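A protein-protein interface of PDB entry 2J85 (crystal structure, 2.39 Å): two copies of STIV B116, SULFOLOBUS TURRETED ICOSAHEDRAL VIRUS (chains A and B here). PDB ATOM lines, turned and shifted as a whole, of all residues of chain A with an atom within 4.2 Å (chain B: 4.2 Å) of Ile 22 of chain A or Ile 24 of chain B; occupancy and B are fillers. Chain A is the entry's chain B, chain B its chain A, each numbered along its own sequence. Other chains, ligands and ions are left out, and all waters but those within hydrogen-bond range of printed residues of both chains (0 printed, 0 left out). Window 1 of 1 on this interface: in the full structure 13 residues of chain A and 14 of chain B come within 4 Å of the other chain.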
ATOM      1  N   PHE A  10     -10.196 -21.545  25.334  1.00  0.00           N
ATOM      2  CA  PHE A  10      -9.563 -21.011  24.135  1.00  0.00           C
ATOM      3  C   PHE A  10     -10.195 -19.673  23.806  1.00  0.00           C
ATOM      4  O   PHE A  10     -11.401 -19.517  23.847  1.00  0.00           O
ATOM      5  CB  PHE A  10      -9.607 -21.924  22.911  1.00  0.00           C
ATOM      6  CG  PHE A  10      -8.989 -21.273  21.708  1.00  0.00           C
ATOM      7  CD1 PHE A  10      -7.616 -21.116  21.630  1.00  0.00           C
ATOM      8  CD2 PHE A  10      -9.781 -20.679  20.739  1.00  0.00           C
ATOM      9  CE1 PHE A  10      -7.041 -20.445  20.545  1.00  0.00           C
ATOM     10  CE2 PHE A  10      -9.217 -20.008  19.658  1.00  0.00           C
ATOM     11  CZ  PHE A  10      -7.847 -19.878  19.570  1.00  0.00           C
ATOM     12  N   LEU A  15      -3.932 -15.601  20.467  1.00  0.00           N
ATOM     13  CA  LEU A  15      -3.185 -15.659  19.217  1.00  0.00           C
ATOM     14  C   LEU A  15      -2.416 -14.347  19.077  1.00  0.00           C
ATOM     15  O   LEU A  15      -2.967 -13.261  19.273  1.00  0.00           O
ATOM     16  CB  LEU A  15      -4.125 -15.912  18.030  1.00  0.00           C
ATOM     17  CG  LEU A  15      -5.038 -17.148  18.173  1.00  0.00           C
ATOM     18  CD1 LEU A  15      -6.174 -17.154  17.141  1.00  0.00           C
ATOM     19  CD2 LEU A  15      -4.243 -18.448  18.105  1.00  0.00           C
ATOM     20  N   PHE A  18      -2.115 -12.081  13.254  1.00  0.00           N
ATOM     21  CA  PHE A  18      -3.187 -12.378  12.325  1.00  0.00           C
ATOM     22  C   PHE A  18      -2.770 -11.899  10.939  1.00  0.00           C
ATOM     23  O   PHE A  18      -2.078 -10.890  10.825  1.00  0.00           O
ATOM     24  CB  PHE A  18      -4.474 -11.684  12.754  1.00  0.00           C
ATOM     25  CG  PHE A  18      -4.868 -11.959  14.173  1.00  0.00           C
ATOM     26  CD1 PHE A  18      -4.436 -11.129  15.195  1.00  0.00           C
ATOM     27  CD2 PHE A  18      -5.668 -13.044  14.486  1.00  0.00           C
ATOM     28  CE1 PHE A  18      -4.802 -11.366  16.511  1.00  0.00           C
ATOM     29  CE2 PHE A  18      -6.035 -13.299  15.789  1.00  0.00           C
ATOM     30  CZ  PHE A  18      -5.601 -12.448  16.812  1.00  0.00           C
ATOM     31  N   PRO A  19      -3.181 -12.626   9.879  1.00  0.00           N
ATOM     32  CA  PRO A  19      -3.984 -13.856   9.956  1.00  0.00           C
ATOM     33  C   PRO A  19      -3.217 -15.077  10.487  1.00  0.00           C
ATOM     34  O   PRO A  19      -1.984 -15.129  10.419  1.00  0.00           O
ATOM     35  CB  PRO A  19      -4.420 -14.089   8.500  1.00  0.00           C
ATOM     36  CG  PRO A  19      -3.357 -13.426   7.662  1.00  0.00           C
ATOM     37  CD  PRO A  19      -2.877 -12.238   8.483  1.00  0.00           C
ATOM     38  N   THR A  20      -3.960 -16.029  11.041  1.00  0.00           N
ATOM     39  CA  THR A  20      -3.413 -17.311  11.426  1.00  0.00           C
ATOM     40  C   THR A  20      -4.446 -18.408  11.189  1.00  0.00           C
ATOM     41  O   THR A  20      -5.674 -18.175  11.199  1.00  0.00           O
ATOM     42  CB  THR A  20      -2.941 -17.333  12.917  1.00  0.00           C
ATOM     43  OG1 THR A  20      -2.071 -18.445  13.107  1.00  0.00           O
ATOM     44  CG2 THR A  20      -4.118 -17.384  13.910  1.00  0.00           C
ATOM     45  N   THR A  21      -3.925 -19.600  10.944  1.00  0.00           N
ATOM     46  CA  THR A  21      -4.729 -20.771  10.653  1.00  0.00           C
ATOM     47  C   THR A  21      -4.366 -21.829  11.682  1.00  0.00           C
ATOM     48  O   THR A  21      -3.167 -22.164  11.874  1.00  0.00           O
ATOM     49  CB  THR A  21      -4.448 -21.254   9.225  1.00  0.00           C
ATOM     50  OG1 THR A  21      -4.783 -20.200   8.317  1.00  0.00           O
ATOM     51  CG2 THR A  21      -5.245 -22.476   8.901  1.00  0.00           C
ATOM     52  N   ILE A  22      -5.403 -22.314  12.369  1.00  0.00           N
ATOM     53  CA  ILE A  22      -5.246 -23.254  13.451  1.00  0.00           C
ATOM     54  C   ILE A  22      -6.131 -24.475  13.245  1.00  0.00           C
ATOM     55  O   ILE A  22      -7.237 -24.370  12.708  1.00  0.00           O
ATOM     56  CB  ILE A  22      -5.544 -22.617  14.847  1.00  0.00           C
ATOM     57  CG1 ILE A  22      -6.985 -22.098  14.940  1.00  0.00           C
ATOM     58  CG2 ILE A  22      -4.491 -21.525  15.171  1.00  0.00           C
ATOM     59  CD1 ILE A  22      -7.411 -21.533  16.349  1.00  0.00           C
ATOM     60  N   THR A  23      -5.603 -25.629  13.653  1.00  0.00           N
ATOM     61  CA  THR A  23      -6.341 -26.851  13.723  1.00  0.00           C
ATOM     62  C   THR A  23      -6.669 -27.124  15.183  1.00  0.00           C
ATOM     63  O   THR A  23      -5.834 -26.931  16.064  1.00  0.00           O
ATOM     64  CB  THR A  23      -5.554 -28.019  13.125  1.00  0.00           C
ATOM     65  OG1 THR A  23      -5.190 -27.683  11.788  1.00  0.00           O
ATOM     66  CG2 THR A  23      -6.390 -29.319  13.129  1.00  0.00           C
ATOM     67  N   ILE A  24      -7.908 -27.558  15.396  1.00  0.00           N
ATOM     68  CA  ILE A  24      -8.455 -27.914  16.672  1.00  0.00           C
ATOM     69  C   ILE A  24      -8.984 -29.358  16.595  1.00  0.00           C
ATOM     70  O   ILE A  24      -9.800 -29.672  15.711  1.00  0.00           O
ATOM     71  CB  ILE A  24      -9.622 -26.960  17.047  1.00  0.00           C
ATOM     72  CG1 ILE A  24      -9.128 -25.503  17.024  1.00  0.00           C
ATOM     73  CG2 ILE A  24     -10.193 -27.302  18.411  1.00  0.00           C
ATOM     74  CD1 ILE A  24     -10.194 -24.499  17.306  1.00  0.00           C
ATOM     75  N   VAL A 115      -5.112 -27.431  20.302  1.00  0.00           N
ATOM     76  CA  VAL A 115      -5.058 -26.387  19.293  1.00  0.00           C
ATOM     77  C   VAL A 115      -3.609 -26.232  18.881  1.00  0.00           C
ATOM     78  O   VAL A 115      -2.759 -26.001  19.713  1.00  0.00           O
ATOM     79  CB  VAL A 115      -5.562 -25.022  19.819  1.00  0.00           C
ATOM     80  CG1 VAL A 115      -5.452 -23.913  18.709  1.00  0.00           C
ATOM     81  CG2 VAL A 115      -7.003 -25.128  20.344  1.00  0.00           C
ATOM     82  N   TRP A 116      -3.342 -26.382  17.591  1.00  0.00           N
ATOM     83  CA  TRP A 116      -2.047 -26.133  17.036  1.00  0.00           C
ATOM     84  C   TRP A 116      -2.218 -25.448  15.698  1.00  0.00           C
ATOM     85  O   TRP A 116      -3.326 -25.366  15.177  1.00  0.00           O
ATOM     86  CB  TRP A 116      -1.275 -27.429  16.885  1.00  0.00           C
ATOM     87  CG  TRP A 116      -1.802 -28.375  15.839  1.00  0.00           C
ATOM     88  CD1 TRP A 116      -1.353 -28.513  14.529  1.00  0.00           C
ATOM     89  CD2 TRP A 116      -2.817 -29.360  16.015  1.00  0.00           C
ATOM     90  NE1 TRP A 116      -2.060 -29.502  13.895  1.00  0.00           N
ATOM     91  CE2 TRP A 116      -2.961 -30.041  14.779  1.00  0.00           C
ATOM     92  CE3 TRP A 116      -3.630 -29.723  17.081  1.00  0.00           C
ATOM     93  CZ2 TRP A 116      -3.877 -31.072  14.603  1.00  0.00           C
ATOM     94  CZ3 TRP A 116      -4.568 -30.735  16.901  1.00  0.00           C
ATOM     95  CH2 TRP A 116      -4.681 -31.400  15.682  1.00  0.00           C
ATOM     96  N   HIS A 117      -1.110 -24.931  15.175  1.00  0.00           N
ATOM     97  CA  HIS A 117      -1.103 -24.183  13.919  1.00  0.00           C
ATOM     98  C   HIS A 117      -0.951 -25.128  12.751  1.00  0.00           C
ATOM     99  O   HIS A 117      -0.117 -26.045  12.807  1.00  0.00           O
ATOM    100  CB  HIS A 117       0.005 -23.128  13.958  1.00  0.00           C
ATOM    101  CG  HIS A 117      -0.253 -22.041  14.965  1.00  0.00           C
ATOM    102  ND1 HIS A 117       0.002 -22.191  16.313  1.00  0.00           N
ATOM    103  CD2 HIS A 117      -0.791 -20.803  14.824  1.00  0.00           C
ATOM    104  CE1 HIS A 117      -0.346 -21.086  16.951  1.00  0.00           C
ATOM    105  NE2 HIS A 117      -0.822 -20.226  16.068  1.00  0.00           N
ATOM    106  N   THR B  20     -11.182 -29.743  13.012  1.00  0.00           N
ATOM    107  CA  THR B  20     -11.402 -28.718  11.999  1.00  0.00           C
ATOM    108  C   THR B  20     -10.264 -27.675  11.959  1.00  0.00           C
ATOM    109  O   THR B  20      -9.495 -27.527  12.906  1.00  0.00           O
ATOM    110  CB  THR B  20     -12.797 -28.054  12.172  1.00  0.00           C
ATOM    111  OG1 THR B  20     -13.034 -27.155  11.087  1.00  0.00           O
ATOM    112  CG2 THR B  20     -12.923 -27.303  13.525  1.00  0.00           C
ATOM    113  N   THR B  21     -10.162 -26.968  10.843  1.00  0.00           N
ATOM    114  CA  THR B  21      -9.067 -26.027  10.591  1.00  0.00           C
ATOM    115  C   THR B  21      -9.696 -24.708  10.158  1.00  0.00           C
ATOM    116  O   THR B  21     -10.447 -24.661   9.180  1.00  0.00           O
ATOM    117  CB  THR B  21      -8.088 -26.584   9.500  1.00  0.00           C
ATOM    118  OG1 THR B  21      -7.579 -27.854   9.931  1.00  0.00           O
ATOM    119  CG2 THR B  21      -6.907 -25.645   9.247  1.00  0.00           C
ATOM    120  N   ILE B  22      -9.418 -23.652  10.913  1.00  0.00           N
ATOM    121  CA  ILE B  22     -10.025 -22.363  10.673  1.00  0.00           C
ATOM    122  C   ILE B  22      -8.986 -21.264  10.569  1.00  0.00           C
ATOM    123  O   ILE B  22      -7.897 -21.345  11.160  1.00  0.00           O
ATOM    124  CB  ILE B  22     -11.047 -22.014  11.774  1.00  0.00           C
ATOM    125  CG1 ILE B  22     -10.394 -22.026  13.171  1.00  0.00           C
ATOM    126  CG2 ILE B  22     -12.231 -23.007  11.707  1.00  0.00           C
ATOM    127  CD1 ILE B  22     -11.300 -21.438  14.316  1.00  0.00           C
ATOM    128  N   THR B  23      -9.325 -20.245   9.797  1.00  0.00           N
ATOM    129  CA  THR B  23      -8.491 -19.102   9.648  1.00  0.00           C
ATOM    130  C   THR B  23      -9.205 -17.946  10.332  1.00  0.00           C
ATOM    131  O   THR B  23     -10.432 -17.808  10.265  1.00  0.00           O
ATOM    132  CB  THR B  23      -8.162 -18.828   8.154  1.00  0.00           C
ATOM    133  OG1 THR B  23      -7.372 -19.916   7.631  1.00  0.00           O
ATOM    134  CG2 THR B  23      -7.409 -17.507   7.987  1.00  0.00           C
ATOM    135  N   ILE B  24      -8.399 -17.157  11.036  1.00  0.00           N
ATOM    136  CA  ILE B  24      -8.855 -16.022  11.804  1.00  0.00           C
ATOM    137  C   ILE B  24      -8.038 -14.824  11.349  1.00  0.00           C
ATOM    138  O   ILE B  24      -6.804 -14.874  11.404  1.00  0.00           O
ATOM    139  CB  ILE B  24      -8.630 -16.227  13.326  1.00  0.00           C
ATOM    140  CG1 ILE B  24      -9.378 -17.474  13.822  1.00  0.00           C
ATOM    141  CG2 ILE B  24      -9.104 -14.986  14.100  1.00  0.00           C
ATOM    142  CD1 ILE B  24      -8.783 -18.132  15.043  1.00  0.00           C
ATOM    143  N   ASP B  25      -8.704 -13.755  10.906  1.00  0.00           N
ATOM    144  CA  ASP B  25      -7.994 -12.473  10.671  1.00  0.00           C
ATOM    145  C   ASP B  25      -8.573 -11.384  11.563  1.00  0.00           C
ATOM    146  O   ASP B  25      -9.724 -11.442  11.956  1.00  0.00           O
ATOM    147  CB  ASP B  25      -8.078 -12.033   9.185  1.00  0.00           C
ATOM    148  CG  ASP B  25      -6.869 -11.133   8.734  1.00  0.00           C
ATOM    149  OD1 ASP B  25      -5.997 -10.739   9.561  1.00  0.00           O
ATOM    150  OD2 ASP B  25      -6.798 -10.825   7.512  1.00  0.00           O
ATOM    151  N   GLU B 114     -12.684 -12.023  11.825  1.00  0.00           N
ATOM    152  CA  GLU B 114     -13.474 -12.859  10.974  1.00  0.00           C
ATOM    153  C   GLU B 114     -12.901 -14.255  11.106  1.00  0.00           C
ATOM    154  O   GLU B 114     -11.679 -14.417  11.088  1.00  0.00           O
ATOM    155  CB  GLU B 114     -13.407 -12.353   9.545  1.00  0.00           C
ATOM    156  CG  GLU B 114     -14.310 -13.102   8.606  1.00  0.00           C
ATOM    157  CD  GLU B 114     -14.265 -12.545   7.208  1.00  0.00           C
ATOM    158  OE1 GLU B 114     -13.380 -11.689   6.904  1.00  0.00           O
ATOM    159  OE2 GLU B 114     -15.124 -12.969   6.408  1.00  0.00           O
ATOM    160  N   VAL B 115     -13.776 -15.250  11.219  1.00  0.00           N
ATOM    161  CA  VAL B 115     -13.350 -16.629  11.336  1.00  0.00           C
ATOM    162  C   VAL B 115     -14.042 -17.383  10.226  1.00  0.00           C
ATOM    163  O   VAL B 115     -15.263 -17.296  10.082  1.00  0.00           O
ATOM    164  CB  VAL B 115     -13.701 -17.220  12.734  1.00  0.00           C
ATOM    165  CG1 VAL B 115     -13.269 -18.663  12.866  1.00  0.00           C
ATOM    166  CG2 VAL B 115     -13.083 -16.331  13.831  1.00  0.00           C
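Thr 21 of chain B touches its own counterpart, Thr 21 of chain A. Thr 21 of chain A touches Thr 23 of chain B, and with the chains exchanged Thr 23 of chain A touches Thr 21 of chain B. Ile 22 of chain B touches its own counterpart, Ile 22 of chain A. Ile 22 of chain A touches Ile 24 of chain B, but with the chains exchanged Ile 24 of chain A does not touch Ile 22 of chain B (4.4 Å). Of the 18 pairs that touch across the chains among the printed residues, 12 have their exchanged pair printed and touching as well.
The backbone carbonyl oxygen of Thr 20 of chain B sits at hydrogen-bond distance from the backbone NH of Ile 24 of chain A (3.0 Å). The side-chain hydroxyl (OG1) of Thr 21 of chain B lies within hydrogen-bond range of the side-chain hydroxyl (OG1) of Thr 23 of chain A (3.0 Å). The backbone carbonyl oxygen (O) of Ile 22 of chain A lies within hydrogen-bond range of the backbone NH (N) of Ile 22 of chain B, at 2.9 Å. The side-chain hydroxyl of Thr 23 of chain B sits at hydrogen-bond distance from the side-chain hydroxyl of Thr 21 of chain A, 2.7 Å away. The backbone NH of Ile 24 of chain B sits at hydrogen-bond distance from the backbone carbonyl oxygen of Thr 20 of chain A, 2.9 Å away. N of Pro 19 of chain A sits close to OD1 of Asp 25 of chain B, 3.4 Å away.
O of Asp 25 of chain B is in hydrogen-bond range of N of Glu 114 of chain B (3.0 Å). The backbone carbonyl oxygen of Trp 116 of chain A is in hydrogen-bond range of the backbone NH of Thr 23 of chain A (2.8 Å).
Printed residues of chain A that touch a printed residue of chain B: Leu 15, Phe 18, Pro 19, Thr 20, Thr 21, Ile 22, Thr 23 and Ile 24. Hydrophobic or aromatic side chains of chain A within 4 Å of the printed part of chain B: Leu 15, Phe 18, Pro 19 and Ile 22. Printed residues of chain B that touch a printed residue of chain A: Thr 20, Thr 21, Ile 22, Thr 23, Ile 24 and Asp 25. Among the printed residues, no Asp or Glu carboxylate lies within 4 Å of a Lys or Arg side-chain nitrogen of the other chain.
Ile 22 of chain A touches just these residues of chain B: Thr 20, Thr 21, Ile 22 and Ile 24. Ile 24 of chain B touches just these residues of chain A: Leu 15, Phe 18, Pro 19, Thr 20 and Ile 22. Of the printed residues of chain B, Thr 23 of chain A touches Thr 20 (3.3 Å) and Thr 21 (3.0 Å). Of the printed residues of chain A, Ile 22 of chain B touches Thr 20 (3.9 Å), Thr 21 (3.3 Å) and Ile 22 (2.9 Å). Of the printed residues of chain B, Pro 19 of chain A touches Ile 24 (3.3 Å) and Asp 25 (3.4 Å). Trp 116 of chain A touches none of the printed residues of chain B. The nearest printed residue of chain B that does not touch Ile 22 of chain A is Thr 23 of chain B (5.1 Å).
Among the printed residues, merely in contact across the chains: Ile 22 of chain A with Thr 21 of chain B (3.3 Å), Thr 21 of chain A with Ile 22 of chain B (3.3 Å), Thr 23 of chain A with Thr 20 of chain B (3.3 Å), Pro 19 of chain A with Ile 24 of chain B (3.3 Å), Thr 20 of chain A with Thr 23 of chain B (3.3 Å), Leu 15 of chain A with Ile 24 of chain B (3.5 Å), Thr 21 of chain A with Thr 21 of chain B (3.6 Å), Phe 18 of chain A with Asp 25 of chain B (3.7 Å), Phe 18 of chain A with Ile 24 of chain B (3.8 Å), Thr 20 of chain A with Ile 22 of chain B (3.9 Å), Ile 22 of chain A with Thr 20 of chain B (3.9 Å) and Ile 22 of chain A with Ile 24 of chain B (3.9 Å).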
